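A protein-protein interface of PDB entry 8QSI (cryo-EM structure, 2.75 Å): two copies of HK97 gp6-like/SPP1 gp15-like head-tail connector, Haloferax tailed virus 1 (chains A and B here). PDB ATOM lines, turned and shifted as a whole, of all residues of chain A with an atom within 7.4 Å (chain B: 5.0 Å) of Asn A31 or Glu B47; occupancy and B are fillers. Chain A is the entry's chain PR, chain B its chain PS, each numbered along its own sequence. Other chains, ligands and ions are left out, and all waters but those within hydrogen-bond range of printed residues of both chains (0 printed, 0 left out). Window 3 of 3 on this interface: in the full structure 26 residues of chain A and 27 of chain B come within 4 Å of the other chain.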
ATOM      1  N   PRO A   2     -18.379  10.348  25.562  1.00  0.00           N
ATOM      2  CA  PRO A   2     -18.833   9.031  25.094  1.00  0.00           C
ATOM      3  C   PRO A   2     -18.834   7.983  26.205  1.00  0.00           C
ATOM      4  O   PRO A   2     -18.027   8.067  27.130  1.00  0.00           O
ATOM      5  CB  PRO A   2     -17.851   8.704  23.959  1.00  0.00           C
ATOM      6  CG  PRO A   2     -17.658  10.049  23.306  1.00  0.00           C
ATOM      7  CD  PRO A   2     -17.619  10.998  24.488  1.00  0.00           C
ATOM      8  N   ASP A  24     -20.436   7.891  18.367  1.00  0.00           N
ATOM      9  CA  ASP A  24     -20.337   8.781  19.511  1.00  0.00           C
ATOM     10  C   ASP A  24     -18.915   9.335  19.669  1.00  0.00           C
ATOM     11  O   ASP A  24     -18.729  10.535  19.870  1.00  0.00           O
ATOM     12  CB  ASP A  24     -20.797   8.017  20.748  1.00  0.00           C
ATOM     13  CG  ASP A  24     -21.133   8.884  21.943  1.00  0.00           C
ATOM     14  OD1 ASP A  24     -21.405  10.089  21.755  1.00  0.00           O
ATOM     15  OD2 ASP A  24     -21.149   8.334  23.068  1.00  0.00           O
ATOM     16  N   ILE A  25     -17.898   8.483  19.520  1.00  0.00           N
ATOM     17  CA  ILE A  25     -16.505   8.918  19.521  1.00  0.00           C
ATOM     18  C   ILE A  25     -16.180   9.733  18.264  1.00  0.00           C
ATOM     19  O   ILE A  25     -15.524  10.765  18.369  1.00  0.00           O
ATOM     20  CB  ILE A  25     -15.544   7.729  19.739  1.00  0.00           C
ATOM     21  CG1 ILE A  25     -15.714   7.150  21.143  1.00  0.00           C
ATOM     22  CG2 ILE A  25     -14.097   8.128  19.488  1.00  0.00           C
ATOM     23  CD1 ILE A  25     -15.006   5.824  21.373  1.00  0.00           C
ATOM     24  N   ILE A  26     -16.642   9.307  17.081  1.00  0.00           N
ATOM     25  CA  ILE A  26     -16.461  10.059  15.843  1.00  0.00           C
ATOM     26  C   ILE A  26     -17.035  11.470  15.988  1.00  0.00           C
ATOM     27  O   ILE A  26     -16.365  12.439  15.645  1.00  0.00           O
ATOM     28  CB  ILE A  26     -17.034   9.301  14.626  1.00  0.00           C
ATOM     29  CG1 ILE A  26     -16.203   8.056  14.311  1.00  0.00           C
ATOM     30  CG2 ILE A  26     -17.120  10.200  13.397  1.00  0.00           C
ATOM     31  CD1 ILE A  26     -16.945   6.973  13.556  1.00  0.00           C
ATOM     32  N   SER A  27     -18.241  11.593  16.556  1.00  0.00           N
ATOM     33  CA  SER A  27     -18.877  12.865  16.857  1.00  0.00           C
ATOM     34  C   SER A  27     -17.996  13.733  17.758  1.00  0.00           C
ATOM     35  O   SER A  27     -17.856  14.929  17.517  1.00  0.00           O
ATOM     36  CB  SER A  27     -20.230  12.626  17.458  1.00  0.00           C
ATOM     37  OG  SER A  27     -20.860  13.851  17.791  1.00  0.00           O
ATOM     38  N   GLN A  28     -17.355  13.134  18.764  1.00  0.00           N
ATOM     39  CA  GLN A  28     -16.445  13.877  19.619  1.00  0.00           C
ATOM     40  C   GLN A  28     -15.235  14.399  18.834  1.00  0.00           C
ATOM     41  O   GLN A  28     -14.866  15.558  18.997  1.00  0.00           O
ATOM     42  CB  GLN A  28     -16.045  13.060  20.841  1.00  0.00           C
ATOM     43  CG  GLN A  28     -15.338  13.926  21.870  1.00  0.00           C
ATOM     44  CD  GLN A  28     -14.854  13.213  23.109  1.00  0.00           C
ATOM     45  OE1 GLN A  28     -14.792  11.984  23.165  1.00  0.00           O
ATOM     46  NE2 GLN A  28     -14.493  13.995  24.125  1.00  0.00           N
ATOM     47  N   VAL A  29     -14.624  13.586  17.966  1.00  0.00           N
ATOM     48  CA  VAL A  29     -13.489  14.037  17.167  1.00  0.00           C
ATOM     49  C   VAL A  29     -13.900  15.164  16.221  1.00  0.00           C
ATOM     50  O   VAL A  29     -13.159  16.134  16.082  1.00  0.00           O
ATOM     51  CB  VAL A  29     -12.786  12.886  16.425  1.00  0.00           C
ATOM     52  CG1 VAL A  29     -11.708  13.385  15.472  1.00  0.00           C
ATOM     53  CG2 VAL A  29     -12.152  11.934  17.415  1.00  0.00           C
ATOM     54  N   GLU A  30     -15.082  15.078  15.605  1.00  0.00           N
ATOM     55  CA  GLU A  30     -15.584  16.130  14.734  1.00  0.00           C
ATOM     56  C   GLU A  30     -15.707  17.483  15.444  1.00  0.00           C
ATOM     57  O   GLU A  30     -15.653  18.511  14.782  1.00  0.00           O
ATOM     58  CB  GLU A  30     -16.923  15.725  14.138  1.00  0.00           C
ATOM     59  CG  GLU A  30     -16.827  14.611  13.113  1.00  0.00           C
ATOM     60  CD  GLU A  30     -18.175  14.153  12.570  1.00  0.00           C
ATOM     61  OE1 GLU A  30     -19.208  14.385  13.238  1.00  0.00           O
ATOM     62  OE2 GLU A  30     -18.205  13.581  11.465  1.00  0.00           O
ATOM     63  N   ASN A  31     -15.852  17.518  16.774  1.00  0.00           N
ATOM     64  CA  ASN A  31     -15.880  18.773  17.513  1.00  0.00           C
ATOM     65  C   ASN A  31     -14.534  19.507  17.490  1.00  0.00           C
ATOM     66  O   ASN A  31     -14.488  20.671  17.877  1.00  0.00           O
ATOM     67  CB  ASN A  31     -16.303  18.573  18.969  1.00  0.00           C
ATOM     68  CG  ASN A  31     -17.734  18.107  19.132  1.00  0.00           C
ATOM     69  OD1 ASN A  31     -18.563  18.303  18.243  1.00  0.00           O
ATOM     70  ND2 ASN A  31     -18.032  17.512  20.277  1.00  0.00           N
ATOM     71  N   LEU A  32     -13.448  18.870  17.039  1.00  0.00           N
ATOM     72  CA  LEU A  32     -12.146  19.527  17.006  1.00  0.00           C
ATOM     73  C   LEU A  32     -11.923  20.356  15.734  1.00  0.00           C
ATOM     74  O   LEU A  32     -10.875  20.972  15.581  1.00  0.00           O
ATOM     75  CB  LEU A  32     -11.031  18.503  17.222  1.00  0.00           C
ATOM     76  CG  LEU A  32     -11.119  17.719  18.528  1.00  0.00           C
ATOM     77  CD1 LEU A  32      -9.917  16.805  18.661  1.00  0.00           C
ATOM     78  CD2 LEU A  32     -11.211  18.636  19.735  1.00  0.00           C
ATOM     79  N   SER A  33     -12.903  20.417  14.830  1.00  0.00           N
ATOM     80  CA  SER A  33     -12.861  21.347  13.715  1.00  0.00           C
ATOM     81  C   SER A  33     -14.193  22.080  13.588  1.00  0.00           C
ATOM     82  O   SER A  33     -15.255  21.476  13.735  1.00  0.00           O
ATOM     83  CB  SER A  33     -12.511  20.639  12.448  1.00  0.00           C
ATOM     84  OG  SER A  33     -12.590  21.563  11.378  1.00  0.00           O
ATOM     85  N   SER A  34     -14.127  23.374  13.258  1.00  0.00           N
ATOM     86  CA  SER A  34     -15.309  24.172  12.958  1.00  0.00           C
ATOM     87  C   SER A  34     -16.080  23.605  11.763  1.00  0.00           C
ATOM     88  O   SER A  34     -17.307  23.695  11.732  1.00  0.00           O
ATOM     89  CB  SER A  34     -14.944  25.611  12.731  1.00  0.00           C
ATOM     90  OG  SER A  34     -13.914  25.692  11.759  1.00  0.00           O
ATOM     91  N   GLY A  36     -15.946  20.335  10.967  1.00  0.00           N
ATOM     92  CA  GLY A  36     -16.242  18.944  11.276  1.00  0.00           C
ATOM     93  C   GLY A  36     -15.789  17.939  10.215  1.00  0.00           C
ATOM     94  O   GLY A  36     -16.139  16.767  10.322  1.00  0.00           O
ATOM     95  N   TRP A  37     -15.039  18.385   9.194  1.00  0.00           N
ATOM     96  CA  TRP A  37     -14.687  17.573   8.033  1.00  0.00           C
ATOM     97  C   TRP A  37     -15.909  16.836   7.458  1.00  0.00           C
ATOM     98  O   TRP A  37     -15.832  15.639   7.170  1.00  0.00           O
ATOM     99  CB  TRP A  37     -13.546  16.602   8.384  1.00  0.00           C
ATOM    100  CG  TRP A  37     -12.353  17.210   9.055  1.00  0.00           C
ATOM    101  CD1 TRP A  37     -11.338  17.885   8.450  1.00  0.00           C
ATOM    102  CD2 TRP A  37     -12.030  17.183  10.463  1.00  0.00           C
ATOM    103  NE1 TRP A  37     -10.408  18.266   9.382  1.00  0.00           N
ATOM    104  CE2 TRP A  37     -10.797  17.853  10.634  1.00  0.00           C
ATOM    105  CE3 TRP A  37     -12.650  16.659  11.604  1.00  0.00           C
ATOM    106  CZ2 TRP A  37     -10.189  18.007  11.895  1.00  0.00           C
ATOM    107  CZ3 TRP A  37     -12.055  16.805  12.848  1.00  0.00           C
ATOM    108  CH2 TRP A  37     -10.836  17.480  12.995  1.00  0.00           C
ATOM    109  N   GLU A  75      -7.435  10.955  26.843  1.00  0.00           N
ATOM    110  CA  GLU A  75      -8.600  11.171  25.997  1.00  0.00           C
ATOM    111  C   GLU A  75      -8.269  12.231  24.951  1.00  0.00           C
ATOM    112  O   GLU A  75      -8.237  11.933  23.764  1.00  0.00           O
ATOM    113  CB  GLU A  75      -9.811  11.510  26.864  1.00  0.00           C
ATOM    114  CG  GLU A  75     -11.037  11.983  26.096  1.00  0.00           C
ATOM    115  CD  GLU A  75     -12.174  12.489  26.979  1.00  0.00           C
ATOM    116  OE1 GLU A  75     -11.988  12.565  28.216  1.00  0.00           O
ATOM    117  OE2 GLU A  75     -13.250  12.804  26.440  1.00  0.00           O
ATOM    118  N   TYR A  76      -7.936  13.446  25.393  1.00  0.00           N
ATOM    119  CA  TYR A  76      -7.649  14.534  24.473  1.00  0.00           C
ATOM    120  C   TYR A  76      -6.404  14.293  23.633  1.00  0.00           C
ATOM    121  O   TYR A  76      -6.410  14.673  22.473  1.00  0.00           O
ATOM    122  CB  TYR A  76      -7.696  15.889  25.169  1.00  0.00           C
ATOM    123  CG  TYR A  76      -9.131  16.287  25.383  1.00  0.00           C
ATOM    124  CD1 TYR A  76      -9.921  16.619  24.295  1.00  0.00           C
ATOM    125  CD2 TYR A  76      -9.737  16.226  26.633  1.00  0.00           C
ATOM    126  CE1 TYR A  76     -11.270  16.909  24.436  1.00  0.00           C
ATOM    127  CE2 TYR A  76     -11.078  16.537  26.797  1.00  0.00           C
ATOM    128  CZ  TYR A  76     -11.846  16.883  25.695  1.00  0.00           C
ATOM    129  OH  TYR A  76     -13.174  17.172  25.840  1.00  0.00           O
ATOM    130  N   LEU A  79      -7.797  12.147  20.844  1.00  0.00           N
ATOM    131  CA  LEU A  79      -8.652  12.962  19.995  1.00  0.00           C
ATOM    132  C   LEU A  79      -7.827  13.886  19.101  1.00  0.00           C
ATOM    133  O   LEU A  79      -8.067  13.905  17.902  1.00  0.00           O
ATOM    134  CB  LEU A  79      -9.670  13.740  20.832  1.00  0.00           C
ATOM    135  CG  LEU A  79     -10.638  12.891  21.647  1.00  0.00           C
ATOM    136  CD1 LEU A  79     -11.342  13.752  22.670  1.00  0.00           C
ATOM    137  CD2 LEU A  79     -11.662  12.200  20.756  1.00  0.00           C
ATOM    138  N   TYR A  80      -6.821  14.589  19.630  1.00  0.00           N
ATOM    139  CA  TYR A  80      -5.948  15.415  18.804  1.00  0.00           C
ATOM    140  C   TYR A  80      -5.172  14.574  17.797  1.00  0.00           C
ATOM    141  O   TYR A  80      -5.044  14.962  16.645  1.00  0.00           O
ATOM    142  CB  TYR A  80      -4.977  16.256  19.637  1.00  0.00           C
ATOM    143  CG  TYR A  80      -5.642  17.324  20.464  1.00  0.00           C
ATOM    144  CD1 TYR A  80      -6.572  18.192  19.904  1.00  0.00           C
ATOM    145  CD2 TYR A  80      -5.352  17.455  21.816  1.00  0.00           C
ATOM    146  CE1 TYR A  80      -7.229  19.141  20.672  1.00  0.00           C
ATOM    147  CE2 TYR A  80      -6.008  18.390  22.595  1.00  0.00           C
ATOM    148  CZ  TYR A  80      -6.943  19.239  22.023  1.00  0.00           C
ATOM    149  OH  TYR A  80      -7.572  20.172  22.798  1.00  0.00           O
ATOM    150  N   TYR A 121      -3.315  20.236  15.097  1.00  0.00           N
ATOM    151  CA  TYR A 121      -3.708  19.166  15.995  1.00  0.00           C
ATOM    152  C   TYR A 121      -2.518  18.327  16.448  1.00  0.00           C
ATOM    153  O   TYR A 121      -2.471  17.900  17.596  1.00  0.00           O
ATOM    154  CB  TYR A 121      -4.759  18.299  15.319  1.00  0.00           C
ATOM    155  CG  TYR A 121      -5.932  19.093  14.830  1.00  0.00           C
ATOM    156  CD1 TYR A 121      -6.767  19.711  15.743  1.00  0.00           C
ATOM    157  CD2 TYR A 121      -6.189  19.267  13.476  1.00  0.00           C
ATOM    158  CE1 TYR A 121      -7.835  20.484  15.328  1.00  0.00           C
ATOM    159  CE2 TYR A 121      -7.253  20.049  13.042  1.00  0.00           C
ATOM    160  CZ  TYR A 121      -8.078  20.655  13.978  1.00  0.00           C
ATOM    161  OH  TYR A 121      -9.143  21.415  13.599  1.00  0.00           O
ATOM    162  N   GLU B  43     -21.115  23.194  20.811  1.00  0.00           N
ATOM    163  CA  GLU B  43     -20.334  21.995  21.097  1.00  0.00           C
ATOM    164  C   GLU B  43     -18.835  22.134  20.798  1.00  0.00           C
ATOM    165  O   GLU B  43     -18.022  21.587  21.538  1.00  0.00           O
ATOM    166  CB  GLU B  43     -20.965  20.767  20.451  1.00  0.00           C
ATOM    167  CG  GLU B  43     -21.915  20.064  21.405  1.00  0.00           C
ATOM    168  CD  GLU B  43     -22.917  20.958  22.126  1.00  0.00           C
ATOM    169  OE1 GLU B  43     -23.809  21.506  21.446  1.00  0.00           O
ATOM    170  OE2 GLU B  43     -22.798  21.124  23.370  1.00  0.00           O
ATOM    171  N   ARG B  44     -18.431  22.882  19.757  1.00  0.00           N
ATOM    172  CA  ARG B  44     -17.016  23.170  19.526  1.00  0.00           C
ATOM    173  C   ARG B  44     -16.426  23.924  20.720  1.00  0.00           C
ATOM    174  O   ARG B  44     -15.355  23.579  21.201  1.00  0.00           O
ATOM    175  CB  ARG B  44     -16.782  23.974  18.240  1.00  0.00           C
ATOM    176  CG  ARG B  44     -16.556  23.136  16.987  1.00  0.00           C
ATOM    177  CD  ARG B  44     -17.827  22.518  16.437  1.00  0.00           C
ATOM    178  NE  ARG B  44     -17.579  21.666  15.285  1.00  0.00           N
ATOM    179  CZ  ARG B  44     -18.473  20.846  14.749  1.00  0.00           C
ATOM    180  NH1 ARG B  44     -18.142  20.109  13.706  1.00  0.00           N
ATOM    181  NH2 ARG B  44     -19.692  20.755  15.253  1.00  0.00           N
ATOM    182  N   LYS B  45     -17.154  24.924  21.219  1.00  0.00           N
ATOM    183  CA  LYS B  45     -16.728  25.751  22.333  1.00  0.00           C
ATOM    184  C   LYS B  45     -16.650  24.943  23.622  1.00  0.00           C
ATOM    185  O   LYS B  45     -15.649  25.026  24.325  1.00  0.00           O
ATOM    186  CB  LYS B  45     -17.649  26.956  22.461  1.00  0.00           C
ATOM    187  CG  LYS B  45     -17.564  27.869  21.255  1.00  0.00           C
ATOM    188  CD  LYS B  45     -18.527  29.010  21.323  1.00  0.00           C
ATOM    189  CE  LYS B  45     -18.598  29.757  20.014  1.00  0.00           C
ATOM    190  NZ  LYS B  45     -19.867  30.507  19.844  1.00  0.00           N
ATOM    191  N   ALA B  46     -17.660  24.115  23.895  1.00  0.00           N
ATOM    192  CA  ALA B  46     -17.632  23.202  25.025  1.00  0.00           C
ATOM    193  C   ALA B  46     -16.432  22.245  24.960  1.00  0.00           C
ATOM    194  O   ALA B  46     -15.734  22.083  25.957  1.00  0.00           O
ATOM    195  CB  ALA B  46     -18.954  22.489  25.114  1.00  0.00           C
ATOM    196  N   GLU B  47     -16.131  21.654  23.797  1.00  0.00           N
ATOM    197  CA  GLU B  47     -14.988  20.757  23.640  1.00  0.00           C
ATOM    198  C   GLU B  47     -13.653  21.478  23.870  1.00  0.00           C
ATOM    199  O   GLU B  47     -12.734  20.933  24.488  1.00  0.00           O
ATOM    200  CB  GLU B  47     -15.016  20.111  22.256  1.00  0.00           C
ATOM    201  CG  GLU B  47     -14.275  18.786  22.203  1.00  0.00           C
ATOM    202  CD  GLU B  47     -15.027  17.619  22.831  1.00  0.00           C
ATOM    203  OE1 GLU B  47     -16.208  17.407  22.470  1.00  0.00           O
ATOM    204  OE2 GLU B  47     -14.439  16.928  23.690  1.00  0.00           O
ATOM    205  N   ALA B  48     -13.545  22.720  23.391  1.00  0.00           N
ATOM    206  CA  ALA B  48     -12.373  23.556  23.605  1.00  0.00           C
ATOM    207  C   ALA B  48     -12.166  23.849  25.093  1.00  0.00           C
ATOM    208  O   ALA B  48     -11.055  23.708  25.588  1.00  0.00           O
ATOM    209  CB  ALA B  48     -12.508  24.825  22.808  1.00  0.00           C
ATOM    210  N   ILE B  49     -13.228  24.205  25.819  1.00  0.00           N
ATOM    211  CA  ILE B  49     -13.155  24.501  27.242  1.00  0.00           C
ATOM    212  C   ILE B  49     -12.824  23.242  28.040  1.00  0.00           C
ATOM    213  O   ILE B  49     -11.901  23.257  28.848  1.00  0.00           O
ATOM    214  CB  ILE B  49     -14.450  25.176  27.708  1.00  0.00           C
ATOM    215  CG1 ILE B  49     -14.478  26.597  27.159  1.00  0.00           C
ATOM    216  CG2 ILE B  49     -14.587  25.170  29.227  1.00  0.00           C
ATOM    217  CD1 ILE B  49     -15.863  27.162  27.018  1.00  0.00           C
ATOM    218  N   ARG B  50     -13.523  22.136  27.780  1.00  0.00           N
ATOM    219  CA  ARG B  50     -13.293  20.883  28.477  1.00  0.00           C
ATOM    220  C   ARG B  50     -11.848  20.415  28.308  1.00  0.00           C
ATOM    221  O   ARG B  50     -11.194  20.041  29.277  1.00  0.00           O
ATOM    222  CB  ARG B  50     -14.285  19.839  27.969  1.00  0.00           C
ATOM    223  CG  ARG B  50     -14.257  18.563  28.792  1.00  0.00           C
ATOM    224  CD  ARG B  50     -15.343  17.624  28.334  1.00  0.00           C
ATOM    225  NE  ARG B  50     -15.459  16.409  29.117  1.00  0.00           N
ATOM    226  CZ  ARG B  50     -14.891  15.240  28.852  1.00  0.00           C
ATOM    227  NH1 ARG B  50     -15.146  14.210  29.640  1.00  0.00           N
ATOM    228  NH2 ARG B  50     -14.057  15.101  27.837  1.00  0.00           N
ATOM    229  N   SER B  51     -11.322  20.494  27.088  1.00  0.00           N
ATOM    230  CA  SER B  51      -9.938  20.140  26.825  1.00  0.00           C
ATOM    231  C   SER B  51      -8.934  21.182  27.322  1.00  0.00           C
ATOM    232  O   SER B  51      -7.781  20.834  27.516  1.00  0.00           O
ATOM    233  CB  SER B  51      -9.714  19.857  25.375  1.00  0.00           C
ATOM    234  OG  SER B  51      -9.928  21.028  24.606  1.00  0.00           O
ATOM    235  N   ALA B  52      -9.318  22.449  27.494  1.00  0.00           N
ATOM    236  CA  ALA B  52      -8.461  23.428  28.152  1.00  0.00           C
ATOM    237  C   ALA B  52      -8.354  23.106  29.644  1.00  0.00           C
ATOM    238  O   ALA B  52      -7.254  23.075  30.180  1.00  0.00           O
ATOM    239  CB  ALA B  52      -8.973  24.823  27.893  1.00  0.00           C
ATOM    240  N   PHE B  89      -9.493  25.398  16.235  1.00  0.00           N
ATOM    241  CA  PHE B  89     -10.639  24.743  15.616  1.00  0.00           C
ATOM    242  C   PHE B  89     -11.154  25.541  14.409  1.00  0.00           C
ATOM    243  O   PHE B  89     -11.714  24.956  13.482  1.00  0.00           O
ATOM    244  CB  PHE B  89     -11.758  24.499  16.633  1.00  0.00           C
ATOM    245  CG  PHE B  89     -11.462  23.636  17.842  1.00  0.00           C
ATOM    246  CD1 PHE B  89     -10.224  23.029  18.055  1.00  0.00           C
ATOM    247  CD2 PHE B  89     -12.464  23.405  18.780  1.00  0.00           C
ATOM    248  CE1 PHE B  89      -9.995  22.241  19.182  1.00  0.00           C
ATOM    249  CE2 PHE B  89     -12.238  22.619  19.906  1.00  0.00           C
ATOM    250  CZ  PHE B  89     -10.999  22.048  20.115  1.00  0.00           C
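No position is printed for both chains.
The side-chain hydroxyl (OG) of Ser B51 sits at hydrogen-bond distance from the backbone carbonyl oxygen (O) of Ala B48, at 3.1 Å. The side-chain carboxylate of Glu A75 lies within hydrogen-bond range of the side-chain amide nitrogen of Gln A28. The side-chain hydroxyl (OH) of Tyr A121 sits at hydrogen-bond distance from the backbone carbonyl oxygen (O) of Leu A32. The backbone carbonyl oxygen (O) of Glu B47 lies within hydrogen-bond range of the side-chain hydroxyl (OG) of Ser B51 (2.8 Å).
NE2 of Gln A28 touches NH2 of Arg B50 (3.9 Å). CG of Arg B44 touches O of Asn A31 (3.3 Å). Asn A31 touches Phe B89 (O to CD2, 3.5 Å). CG of Glu B47 touches CD2 of Leu A32, at 3.9 Å. Leu A32 touches Phe B89. Ser A33 touches Phe B89. CA of Gly A36 touches NH1 of Arg B44 (3.3 Å). Ser B51 touches Tyr A76.
Of the printed residues of chain B, Ser A33 touches Arg B44 (2.8 Å) and Phe B89 (3.8 Å). Printed residues of chain B within 4 Å of Gly A36: Arg B44 (3.3 Å). Of the printed residues of chain B, Tyr A76 touches Glu B47 (2.5 Å), Arg B50 (3.0 Å) and Ser B51 (3.4 Å). Tyr A121 touches none of the printed residues of chain B. Printed residues of chain A within 4 Å of Ser B51: Tyr A76 (3.4 Å) and Tyr A80 (3.1 Å). Ala B52 touches none of the printed residues of chain A. The nearest residue of chain A that does not touch Glu B47 is Leu A79 (4.6 Å). The nearest printed residue of chain B that does not touch Glu A75 is Glu B47 (5.1 Å).
The guanidinium group (NH2) of Arg B50 is in hydrogen-bond range of the side-chain hydroxyl (OH) of Tyr A76 (3.0 Å). The side-chain hydroxyl (OH) of Tyr A80 sits at hydrogen-bond distance from the side-chain hydroxyl (OG) of Ser B51, 3.1 Å away. The side-chain carboxylate (OE2) of Glu B47 is in hydrogen-bond range of the side-chain hydroxyl (OH) of Tyr A76, 2.5 Å away. NE2 of Gln A28 sits at hydrogen-bond distance from OE2 of Glu B47. The guanidinium group (NH2) of Arg B50 is in salt-bridge range of the side-chain carboxylate (OE2) of Glu A75 (2.8 Å). The guanidinium group (NH1) of Arg B44 is in hydrogen-bond range of the backbone carbonyl oxygen (O) of Glu A30 (3.1 Å). The side-chain hydroxyl (OG) of Ser A34 lies within hydrogen-bond range of the backbone carbonyl oxygen (O) of Phe B89, 2.9 Å away. The side-chain carboxylate (OE1) of Glu B47 sits at hydrogen-bond distance from the side-chain amide nitrogen (ND2) of Asn A31, 2.9 Å away. The backbone carbonyl oxygen (O) of Ser A33 sits at hydrogen-bond distance from the guanidinium group (NE) of Arg B44 (2.8 Å).
Hydrophobic or aromatic side chains of chain B within 4 Å of the printed part of chain A: Phe B89. Of the 19 printed residues of chain A, 10 touch a printed residue of chain B. Printed residues of chain A that touch a printed residue of chain B: Gln A28, Glu A30, Asn A31, Leu A32, Ser A33, Ser A34, Gly A36, Glu A75, Tyr A76 and Tyr A80. Hydrophobic or aromatic side chains of chain A within 4 Å of the printed part of chain B: Leu A32, Tyr A76 and Tyr A80. Among the printed residues, Asp or Glu carboxylates within 4 Å of a Lys or Arg side-chain nitrogen of the other chain: Glu A75 with Arg B50.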
